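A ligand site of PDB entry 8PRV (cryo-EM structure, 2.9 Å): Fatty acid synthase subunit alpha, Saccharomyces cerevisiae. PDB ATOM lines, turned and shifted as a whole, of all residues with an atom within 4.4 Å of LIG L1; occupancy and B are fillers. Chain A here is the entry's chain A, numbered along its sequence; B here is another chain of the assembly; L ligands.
The backbone NH (N) of Ser 180 of chain B lies close to an oxygen (O7) of LIG L1 (2.9 Å). A side-chain carbon (CB) of Ser 180 of chain B is bonded to an oxygen (O7) of LIG L1 (1.4 Å). The side-chain hydroxyl (OG) of Ser 827 lies within hydrogen-bond range of an oxygen (O1) of LIG L1. The side-chain amide nitrogen of Asn 881 is in hydrogen-bond range of an oxygen (O3) of LIG L1. The backbone NH (N) of Thr 181 of chain B is in hydrogen-bond range of an oxygen (O7) of LIG L1 (2.9 Å). N of Gly 778 lies within hydrogen-bond range of O4 of LIG L1. The side-chain amide nitrogen of Asn 829 lies within hydrogen-bond range of an oxygen (O2) of LIG L1. NE2 of Gln 777 is in hydrogen-bond range of O5 of LIG L1. O13 of LG2 L2 is in hydrogen-bond range of OH of Tyr 839, 2.8 Å away.
The backbone carbonyl oxygen of Ser 180 of chain B sits close to the side-chain amide nitrogen of Asn 184 of chain B (3.5 Å). The backbone NH of Asn 829 is in hydrogen-bond range of the side-chain hydroxyl of Ser 827 (2.7 Å). The side-chain amide oxygen (OD1) of Asn 881 lies within hydrogen-bond range of the guanidinium group (NH2) of Arg 944, at 2.8 Å. The side-chain amide nitrogen (ND2) of Asn 881 lies within hydrogen-bond range of the side-chain sulfur (SD) of Met 878, 3.6 Å away. N of Gly 778 lies within hydrogen-bond range of O of Gly 835 (2.9 Å). ND2 of Asn 829 lies within hydrogen-bond range of OD2 of Asp 836, at 2.8 Å.
O of Leu 877 sits close to S1 of LIG L1, 3.7 Å away. CD of Pro 828 touches O1 of LIG L1 (3.7 Å). Gly 834 touches LIG L1 (O to C8, 3.4 Å). Gly 835 touches LIG L1. OD2 of Asp 836 touches N1 of LIG L1, at 3.6 Å. OH of Tyr 839 touches C2 of LIG L1, at 3.5 Å. Met 878 touches LIG L1 (SD to S1, 3.9 Å). Leu 930 touches LIG L1. NH2 of Arg 944 touches C14 of LIG L1, at 3.6 Å. 16 residues have an atom within 4 Å of LIG L1: Gln 777, Gly 778, Ser 827, Pro 828, Asn 829, Gly 834, Gly 835, Asp 836, Tyr 839, Leu 877, Met 878, Asn 881, Leu 930, Arg 944, Ser 180 of chain B and Thr 181 of chain B.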
ATOM      1  N   GLU A 776      -0.373 -18.339  -1.957  1.00  0.00           N
ATOM      2  CA  GLU A 776       0.848 -19.151  -1.698  1.00  0.00           C
ATOM      3  C   GLU A 776       0.459 -20.144  -0.606  1.00  0.00           C
ATOM      4  O   GLU A 776      -0.016 -19.683   0.460  1.00  0.00           O
ATOM      5  CB  GLU A 776       1.987 -18.279  -1.179  1.00  0.00           C
ATOM      6  CG  GLU A 776       2.419 -17.138  -2.111  1.00  0.00           C
ATOM      7  CD  GLU A 776       3.086 -15.970  -1.382  1.00  0.00           C
ATOM      8  OE1 GLU A 776       2.362 -15.140  -0.776  1.00  0.00           O
ATOM      9  OE2 GLU A 776       4.346 -15.898  -1.397  1.00  0.00           O
ATOM     10  N   GLN A 777       0.584 -21.428  -0.875  1.00  0.00           N
ATOM     11  CA  GLN A 777       0.035 -22.475   0.026  1.00  0.00           C
ATOM     12  C   GLN A 777       1.006 -23.645   0.022  1.00  0.00           C
ATOM     13  O   GLN A 777       1.465 -24.027  -1.078  1.00  0.00           O
ATOM     14  CB  GLN A 777      -1.339 -22.907  -0.476  1.00  0.00           C
ATOM     15  CG  GLN A 777      -2.464 -21.920  -0.164  1.00  0.00           C
ATOM     16  CD  GLN A 777      -3.753 -22.288  -0.871  1.00  0.00           C
ATOM     17  OE1 GLN A 777      -3.789 -22.448  -2.102  1.00  0.00           O
ATOM     18  NE2 GLN A 777      -4.829 -22.418  -0.109  1.00  0.00           N
ATOM     19  N   GLY A 778       1.304 -24.168   1.210  1.00  0.00           N
ATOM     20  CA  GLY A 778       2.308 -25.230   1.436  1.00  0.00           C
ATOM     21  C   GLY A 778       3.682 -24.815   0.973  1.00  0.00           C
ATOM     22  O   GLY A 778       4.404 -25.678   0.423  1.00  0.00           O
ATOM     23  N   SER A 827      -2.504  -7.648   7.869  1.00  0.00           N
ATOM     24  CA  SER A 827      -2.883  -8.959   8.409  1.00  0.00           C
ATOM     25  C   SER A 827      -2.319  -9.124   9.803  1.00  0.00           C
ATOM     26  O   SER A 827      -1.335  -8.469  10.136  1.00  0.00           O
ATOM     27  CB  SER A 827      -2.408 -10.049   7.519  1.00  0.00           C
ATOM     28  OG  SER A 827      -2.466 -11.296   8.177  1.00  0.00           O
ATOM     29  N   PRO A 828      -2.936  -9.954  10.660  1.00  0.00           N
ATOM     30  CA  PRO A 828      -2.277 -10.462  11.866  1.00  0.00           C
ATOM     31  C   PRO A 828      -1.444 -11.740  11.670  1.00  0.00           C
ATOM     32  O   PRO A 828      -0.857 -12.209  12.642  1.00  0.00           O
ATOM     33  CB  PRO A 828      -3.497 -10.783  12.726  1.00  0.00           C
ATOM     34  CG  PRO A 828      -4.463 -11.328  11.713  1.00  0.00           C
ATOM     35  CD  PRO A 828      -4.342 -10.367  10.570  1.00  0.00           C
ATOM     36  N   ASN A 829      -1.427 -12.301  10.465  1.00  0.00           N
ATOM     37  CA  ASN A 829      -0.520 -13.403  10.066  1.00  0.00           C
ATOM     38  C   ASN A 829       0.853 -12.774   9.832  1.00  0.00           C
ATOM     39  O   ASN A 829       1.111 -12.376   8.655  1.00  0.00           O
ATOM     40  CB  ASN A 829      -1.024 -14.143   8.817  1.00  0.00           C
ATOM     41  CG  ASN A 829      -0.136 -15.248   8.299  1.00  0.00           C
ATOM     42  OD1 ASN A 829       0.883 -15.581   8.896  1.00  0.00           O
ATOM     43  ND2 ASN A 829      -0.544 -15.871   7.190  1.00  0.00           N
ATOM     44  N   PHE A 833       0.728 -18.512  10.948  1.00  0.00           N
ATOM     45  CA  PHE A 833       0.149 -19.698  10.251  1.00  0.00           C
ATOM     46  C   PHE A 833       1.225 -20.569   9.619  1.00  0.00           C
ATOM     47  O   PHE A 833       1.032 -21.808   9.594  1.00  0.00           O
ATOM     48  CB  PHE A 833      -0.758 -19.303   9.089  1.00  0.00           C
ATOM     49  CG  PHE A 833      -2.166 -18.892   9.448  1.00  0.00           C
ATOM     50  CD1 PHE A 833      -3.213 -19.809   9.377  1.00  0.00           C
ATOM     51  CD2 PHE A 833      -2.428 -17.585   9.824  1.00  0.00           C
ATOM     52  CE1 PHE A 833      -4.499 -19.401   9.683  1.00  0.00           C
ATOM     53  CE2 PHE A 833      -3.715 -17.187  10.132  1.00  0.00           C
ATOM     54  CZ  PHE A 833      -4.763 -18.104  10.061  1.00  0.00           C
ATOM     55  N   GLY A 834       2.230 -19.943   8.993  1.00  0.00           N
ATOM     56  CA  GLY A 834       3.360 -20.632   8.329  1.00  0.00           C
ATOM     57  C   GLY A 834       2.950 -21.338   7.053  1.00  0.00           C
ATOM     58  O   GLY A 834       1.759 -21.630   6.863  1.00  0.00           O
ATOM     59  N   GLY A 835       3.911 -21.614   6.184  1.00  0.00           N
ATOM     60  CA  GLY A 835       3.676 -22.380   4.940  1.00  0.00           C
ATOM     61  C   GLY A 835       2.994 -21.544   3.884  1.00  0.00           C
ATOM     62  O   GLY A 835       2.376 -22.138   3.004  1.00  0.00           O
ATOM     63  N   ASP A 836       3.160 -20.228   3.919  1.00  0.00           N
ATOM     64  CA  ASP A 836       2.459 -19.255   3.030  1.00  0.00           C
ATOM     65  C   ASP A 836       3.490 -18.344   2.359  1.00  0.00           C
ATOM     66  O   ASP A 836       3.242 -17.151   2.275  1.00  0.00           O
ATOM     67  CB  ASP A 836       1.394 -18.477   3.814  1.00  0.00           C
ATOM     68  CG  ASP A 836       1.902 -17.861   5.126  1.00  0.00           C
ATOM     69  OD1 ASP A 836       3.089 -17.403   5.185  1.00  0.00           O
ATOM     70  OD2 ASP A 836       1.120 -17.850   6.098  1.00  0.00           O
ATOM     71  N   TYR A 839       4.010 -14.252   2.277  1.00  0.00           N
ATOM     72  CA  TYR A 839       2.754 -13.520   2.523  1.00  0.00           C
ATOM     73  C   TYR A 839       3.031 -12.680   3.759  1.00  0.00           C
ATOM     74  O   TYR A 839       3.045 -11.481   3.679  1.00  0.00           O
ATOM     75  CB  TYR A 839       1.565 -14.476   2.627  1.00  0.00           C
ATOM     76  CG  TYR A 839       0.275 -13.828   3.047  1.00  0.00           C
ATOM     77  CD1 TYR A 839      -0.026 -13.659   4.386  1.00  0.00           C
ATOM     78  CD2 TYR A 839      -0.649 -13.379   2.123  1.00  0.00           C
ATOM     79  CE1 TYR A 839      -1.196 -13.038   4.807  1.00  0.00           C
ATOM     80  CE2 TYR A 839      -1.827 -12.771   2.516  1.00  0.00           C
ATOM     81  CZ  TYR A 839      -2.112 -12.592   3.871  1.00  0.00           C
ATOM     82  OH  TYR A 839      -3.260 -11.973   4.297  1.00  0.00           O
ATOM     83  N   ILE A 869      -7.071  -6.741   8.746  1.00  0.00           N
ATOM     84  CA  ILE A 869      -8.281  -7.531   8.393  1.00  0.00           C
ATOM     85  C   ILE A 869      -8.176  -8.852   9.129  1.00  0.00           C
ATOM     86  O   ILE A 869      -7.078  -9.425   9.147  1.00  0.00           O
ATOM     87  CB  ILE A 869      -8.373  -7.713   6.867  1.00  0.00           C
ATOM     88  CG1 ILE A 869      -8.606  -6.377   6.194  1.00  0.00           C
ATOM     89  CG2 ILE A 869      -9.449  -8.695   6.508  1.00  0.00           C
ATOM     90  CD1 ILE A 869      -8.127  -6.315   4.785  1.00  0.00           C
ATOM     91  N   TRP A 871      -9.608 -12.925  10.030  1.00  0.00           N
ATOM     92  CA  TRP A 871     -10.023 -14.170   9.358  1.00  0.00           C
ATOM     93  C   TRP A 871     -11.347 -13.925   8.641  1.00  0.00           C
ATOM     94  O   TRP A 871     -12.318 -13.654   9.305  1.00  0.00           O
ATOM     95  CB  TRP A 871     -10.163 -15.242  10.413  1.00  0.00           C
ATOM     96  CG  TRP A 871     -10.379 -16.618   9.879  1.00  0.00           C
ATOM     97  CD1 TRP A 871     -11.293 -17.064   8.968  1.00  0.00           C
ATOM     98  CD2 TRP A 871      -9.672 -17.750  10.345  1.00  0.00           C
ATOM     99  NE1 TRP A 871     -11.187 -18.420   8.835  1.00  0.00           N
ATOM    100  CE2 TRP A 871     -10.202 -18.868   9.670  1.00  0.00           C
ATOM    101  CE3 TRP A 871      -8.613 -17.915  11.247  1.00  0.00           C
ATOM    102  CZ2 TRP A 871      -9.685 -20.146   9.847  1.00  0.00           C
ATOM    103  CZ3 TRP A 871      -8.096 -19.184  11.413  1.00  0.00           C
ATOM    104  CH2 TRP A 871      -8.636 -20.281  10.728  1.00  0.00           C
ATOM    105  N   LEU A 877      -7.756 -16.631  -0.432  1.00  0.00           N
ATOM    106  CA  LEU A 877      -6.655 -16.866   0.518  1.00  0.00           C
ATOM    107  C   LEU A 877      -7.098 -17.748   1.697  1.00  0.00           C
ATOM    108  O   LEU A 877      -6.209 -18.301   2.339  1.00  0.00           O
ATOM    109  CB  LEU A 877      -6.111 -15.511   1.000  1.00  0.00           C
ATOM    110  CG  LEU A 877      -5.142 -14.854   0.038  1.00  0.00           C
ATOM    111  CD1 LEU A 877      -4.968 -13.395   0.388  1.00  0.00           C
ATOM    112  CD2 LEU A 877      -3.786 -15.545   0.042  1.00  0.00           C
ATOM    113  N   MET A 878      -8.389 -17.893   1.976  1.00  0.00           N
ATOM    114  CA  MET A 878      -8.852 -18.516   3.238  1.00  0.00           C
ATOM    115  C   MET A 878      -9.922 -19.588   3.053  1.00  0.00           C
ATOM    116  O   MET A 878     -10.391 -20.066   4.105  1.00  0.00           O
ATOM    117  CB  MET A 878      -9.388 -17.442   4.187  1.00  0.00           C
ATOM    118  CG  MET A 878      -8.282 -16.667   4.849  1.00  0.00           C
ATOM    119  SD  MET A 878      -7.220 -17.700   5.888  1.00  0.00           S
ATOM    120  CE  MET A 878      -8.066 -17.429   7.443  1.00  0.00           C
ATOM    121  N   ALA A 880      -9.572 -22.664   1.946  1.00  0.00           N
ATOM    122  CA  ALA A 880      -8.949 -23.912   2.446  1.00  0.00           C
ATOM    123  C   ALA A 880      -9.091 -24.047   3.960  1.00  0.00           C
ATOM    124  O   ALA A 880      -9.074 -25.197   4.432  1.00  0.00           O
ATOM    125  CB  ALA A 880      -7.502 -23.958   2.040  1.00  0.00           C
ATOM    126  N   ASN A 881      -9.226 -22.943   4.696  1.00  0.00           N
ATOM    127  CA  ASN A 881      -9.388 -22.957   6.173  1.00  0.00           C
ATOM    128  C   ASN A 881     -10.854 -22.884   6.612  1.00  0.00           C
ATOM    129  O   ASN A 881     -11.113 -22.671   7.791  1.00  0.00           O
ATOM    130  CB  ASN A 881      -8.564 -21.824   6.801  1.00  0.00           C
ATOM    131  CG  ASN A 881      -7.084 -22.091   6.679  1.00  0.00           C
ATOM    132  OD1 ASN A 881      -6.618 -23.142   7.128  1.00  0.00           O
ATOM    133  ND2 ASN A 881      -6.351 -21.173   6.064  1.00  0.00           N
ATOM    134  N   LEU A 930      -8.095 -12.470  16.784  1.00  0.00           N
ATOM    135  CA  LEU A 930      -7.229 -13.535  16.237  1.00  0.00           C
ATOM    136  C   LEU A 930      -5.778 -13.352  16.711  1.00  0.00           C
ATOM    137  O   LEU A 930      -5.074 -14.359  16.741  1.00  0.00           O
ATOM    138  CB  LEU A 930      -7.307 -13.505  14.707  1.00  0.00           C
ATOM    139  CG  LEU A 930      -6.565 -14.646  14.003  1.00  0.00           C
ATOM    140  CD1 LEU A 930      -7.251 -15.972  14.282  1.00  0.00           C
ATOM    141  CD2 LEU A 930      -6.506 -14.398  12.499  1.00  0.00           C
ATOM    142  N   ARG A 944      -7.612 -29.483  12.519  1.00  0.00           N
ATOM    143  CA  ARG A 944      -7.695 -30.069  11.176  1.00  0.00           C
ATOM    144  C   ARG A 944      -7.440 -31.575  11.289  1.00  0.00           C
ATOM    145  O   ARG A 944      -8.197 -32.338  10.679  1.00  0.00           O
ATOM    146  CB  ARG A 944      -6.721 -29.359  10.238  1.00  0.00           C
ATOM    147  CG  ARG A 944      -6.893 -29.735   8.773  1.00  0.00           C
ATOM    148  CD  ARG A 944      -5.702 -29.249   7.978  1.00  0.00           C
ATOM    149  NE  ARG A 944      -5.451 -27.855   8.304  1.00  0.00           N
ATOM    150  CZ  ARG A 944      -6.090 -26.824   7.757  1.00  0.00           C
ATOM    151  NH1 ARG A 944      -7.023 -26.995   6.835  1.00  0.00           N
ATOM    152  NH2 ARG A 944      -5.751 -25.607   8.141  1.00  0.00           N
ATOM    153  N   LYS B 179      -0.185 -33.815   1.096  1.00  0.00           N
ATOM    154  CA  LYS B 179      -0.043 -32.391   0.701  1.00  0.00           C
ATOM    155  C   LYS B 179      -1.271 -31.997  -0.107  1.00  0.00           C
ATOM    156  O   LYS B 179      -1.305 -32.156  -1.329  1.00  0.00           O
ATOM    157  CB  LYS B 179       1.215 -32.165  -0.149  1.00  0.00           C
ATOM    158  CG  LYS B 179       2.534 -32.191   0.609  1.00  0.00           C
ATOM    159  CD  LYS B 179       3.757 -32.560  -0.235  1.00  0.00           C
ATOM    160  CE  LYS B 179       3.849 -31.856  -1.575  1.00  0.00           C
ATOM    161  NZ  LYS B 179       4.042 -30.389  -1.448  1.00  0.00           N
ATOM    162  N   SER B 180      -2.278 -31.484   0.584  1.00  0.00           N
ATOM    163  CA  SER B 180      -3.533 -31.126  -0.058  1.00  0.00           C
ATOM    164  C   SER B 180      -3.441 -30.027  -1.114  1.00  0.00           C
ATOM    165  O   SER B 180      -4.303 -29.925  -1.979  1.00  0.00           O
ATOM    166  CB  SER B 180      -4.486 -30.670   1.019  1.00  0.00           C
ATOM    167  N   THR B 181      -2.408 -29.186  -1.010  1.00  0.00           N
ATOM    168  CA  THR B 181      -2.192 -28.088  -1.943  1.00  0.00           C
ATOM    169  C   THR B 181      -1.986 -28.650  -3.354  1.00  0.00           C
ATOM    170  O   THR B 181      -2.748 -28.262  -4.262  1.00  0.00           O
ATOM    171  CB  THR B 181      -1.002 -27.223  -1.509  1.00  0.00           C
ATOM    172  OG1 THR B 181       0.183 -28.023  -1.575  1.00  0.00           O
ATOM    173  CG2 THR B 181      -1.163 -26.707  -0.096  1.00  0.00           C
ATOM    174  N   ASN B 184      -5.038 -30.381  -4.835  1.00  0.00           N
ATOM    175  CA  ASN B 184      -5.995 -29.364  -5.350  1.00  0.00           C
ATOM    176  C   ASN B 184      -5.491 -28.741  -6.654  1.00  0.00           C
ATOM    177  O   ASN B 184      -6.338 -28.285  -7.443  1.00  0.00           O
ATOM    178  CB  ASN B 184      -6.287 -28.316  -4.276  1.00  0.00           C
ATOM    179  CG  ASN B 184      -7.220 -28.827  -3.182  1.00  0.00           C
ATOM    180  OD1 ASN B 184      -7.890 -29.848  -3.342  1.00  0.00           O
ATOM    181  ND2 ASN B 184      -7.287 -28.110  -2.072  1.00  0.00           N
HETATM  182  C1  LIG L   1      -4.310 -15.016   5.755  1.00  0.00           C
HETATM  183  C2  LIG L   1      -5.434 -14.043   6.036  1.00  0.00           C
HETATM  184  C3  LIG L   1      -5.236 -13.457   7.422  1.00  0.00           C
HETATM  185  C4  LIG L   1      -5.876 -14.116   8.620  1.00  0.00           C
HETATM  186  O1  LIG L   1      -4.562 -12.445   7.520  1.00  0.00           O
HETATM  187  O2  LIG L   1      -3.446 -15.222   6.608  1.00  0.00           O
HETATM  188  O3  LIG L   1      -3.599 -20.811   5.381  1.00  0.00           O
HETATM  189  C5  LIG L   1      -2.480 -20.333   5.363  1.00  0.00           C
HETATM  190  N1  LIG L   1      -2.208 -19.036   5.289  1.00  0.00           N
HETATM  191  C6  LIG L   1      -3.264 -18.046   5.156  1.00  0.00           C
HETATM  192  C7  LIG L   1      -2.924 -16.956   4.140  1.00  0.00           C
HETATM  193  S1  LIG L   1      -4.222 -15.779   4.249  1.00  0.00           S
HETATM  194  C8  LIG L   1      -1.300 -21.261   5.323  1.00  0.00           C
HETATM  195  C9  LIG L   1      -1.142 -21.624   3.832  1.00  0.00           C
HETATM  196  N2  LIG L   1      -2.006 -22.748   3.463  1.00  0.00           N
HETATM  197  C10 LIG L   1      -1.580 -24.012   3.424  1.00  0.00           C
HETATM  198  O4  LIG L   1      -0.424 -24.342   3.642  1.00  0.00           O
HETATM  199  C11 LIG L   1      -2.580 -25.094   3.149  1.00  0.00           C
HETATM  200  O5  LIG L   1      -3.542 -24.640   2.151  1.00  0.00           O
HETATM  201  C12 LIG L   1      -3.207 -25.658   4.469  1.00  0.00           C
HETATM  202  C13 LIG L   1      -2.178 -25.900   5.594  1.00  0.00           C
HETATM  203  C14 LIG L   1      -4.302 -24.738   4.987  1.00  0.00           C
HETATM  204  C15 LIG L   1      -3.745 -27.061   4.166  1.00  0.00           C
HETATM  205  O6  LIG L   1      -4.442 -27.196   2.908  1.00  0.00           O
HETATM  206  P1  LIG L   1      -4.961 -28.674   2.525  1.00  0.00           P
HETATM  207  O7  LIG L   1      -4.091 -29.351   1.388  1.00  0.00           O
HETATM  208  O8  LIG L   1      -4.713 -29.641   3.687  1.00  0.00           O
HETATM  209  O9  LIG L   1      -6.406 -28.577   2.094  1.00  0.00           O
HETATM  210  P1  LG2 L   2      -8.624 -13.116  -2.804  1.00  0.00           P
HETATM  211  O1  LG2 L   2     -10.003 -13.567  -2.545  1.00  0.00           O
HETATM  212  O2  LG2 L   2      -7.574 -14.070  -3.401  1.00  0.00           O
HETATM  213  O3  LG2 L   2      -8.670 -11.873  -3.756  1.00  0.00           O
HETATM  214  C1  LG2 L   2      -7.486 -11.505  -4.455  1.00  0.00           C
HETATM  215  C2  LG2 L   2      -7.885 -11.198  -5.907  1.00  0.00           C
HETATM  216  O4  LG2 L   2      -6.749 -10.652  -6.539  1.00  0.00           O
HETATM  217  C3  LG2 L   2      -8.211 -12.388  -6.764  1.00  0.00           C
HETATM  218  O5  LG2 L   2      -9.610 -12.662  -6.495  1.00  0.00           O
HETATM  219  C4  LG2 L   2      -7.876 -11.916  -8.144  1.00  0.00           C
HETATM  220  O6  LG2 L   2      -9.019 -11.328  -8.785  1.00  0.00           O
HETATM  221  C5  LG2 L   2      -6.910 -10.802  -7.904  1.00  0.00           C
HETATM  222  N1  LG2 L   2      -5.600 -11.055  -8.471  1.00  0.00           N
HETATM  223  C6  LG2 L   2      -4.870 -12.161  -8.398  1.00  0.00           C
HETATM  224  N2  LG2 L   2      -3.712 -12.023  -9.088  1.00  0.00           N
HETATM  225  C7  LG2 L   2      -3.734 -10.780  -9.558  1.00  0.00           C
HETATM  226  C8  LG2 L   2      -2.838 -10.009 -10.346  1.00  0.00           C
HETATM  227  N3  LG2 L   2      -1.691 -10.562 -10.737  1.00  0.00           N
HETATM  228  N4  LG2 L   2      -3.171  -8.762 -10.641  1.00  0.00           N
HETATM  229  C9  LG2 L   2      -4.330  -8.246 -10.233  1.00  0.00           C
HETATM  230  N5  LG2 L   2      -5.242  -8.925  -9.533  1.00  0.00           N
HETATM  231  C10 LG2 L   2      -4.975 -10.164  -9.169  1.00  0.00           C
HETATM  232  O7  LG2 L   2      -7.986 -12.299  -1.609  1.00  0.00           O
HETATM  233  P2  LG2 L   2      -8.880 -11.803  -0.406  1.00  0.00           P
HETATM  234  O8  LG2 L   2      -9.036 -13.115   0.283  1.00  0.00           O
HETATM  235  O9  LG2 L   2     -10.047 -10.938  -0.819  1.00  0.00           O
HETATM  236  O10 LG2 L   2      -7.942 -10.833   0.416  1.00  0.00           O
HETATM  237  C11 LG2 L   2      -7.678  -9.597  -0.201  1.00  0.00           C
HETATM  238  C12 LG2 L   2      -6.613  -8.784   0.479  1.00  0.00           C
HETATM  239  O11 LG2 L   2      -6.974  -8.715   1.854  1.00  0.00           O
HETATM  240  C13 LG2 L   2      -5.244  -9.403   0.358  1.00  0.00           C
HETATM  241  O12 LG2 L   2      -4.300  -8.334   0.245  1.00  0.00           O
HETATM  242  C14 LG2 L   2      -5.071 -10.138   1.652  1.00  0.00           C
HETATM  243  O13 LG2 L   2      -3.768 -10.181   2.188  1.00  0.00           O
HETATM  244  C15 LG2 L   2      -5.877  -9.283   2.589  1.00  0.00           C
HETATM  245  N6  LG2 L   2      -6.332 -10.071   3.699  1.00  0.00           N
HETATM  246  C16 LG2 L   2      -7.191 -11.069   3.514  1.00  0.00           C
HETATM  247  C17 LG2 L   2      -7.612 -11.804   4.599  1.00  0.00           C
HETATM  248  C18 LG2 L   2      -8.571 -12.892   4.324  1.00  0.00           C
HETATM  249  O14 LG2 L   2      -8.880 -13.187   3.178  1.00  0.00           O
HETATM  250  N7  LG2 L   2      -9.134 -13.510   5.301  1.00  0.00           N
HETATM  251  C19 LG2 L   2      -7.171 -11.497   5.887  1.00  0.00           C
HETATM  252  C20 LG2 L   2      -6.268 -10.448   6.046  1.00  0.00           C
HETATM  253  C21 LG2 L   2      -5.863  -9.738   4.914  1.00  0.00           C
HETATM  254  P3  LG2 L   2      -9.308 -11.302 -10.405  1.00  0.00           P
HETATM  255  O15 LG2 L   2      -9.861 -12.686 -10.653  1.00  0.00           O
HETATM  256  O16 LG2 L   2     -10.277 -10.100 -10.457  1.00  0.00           O
HETATM  257  O17 LG2 L   2      -7.982 -11.171 -11.128  1.00  0.00           O
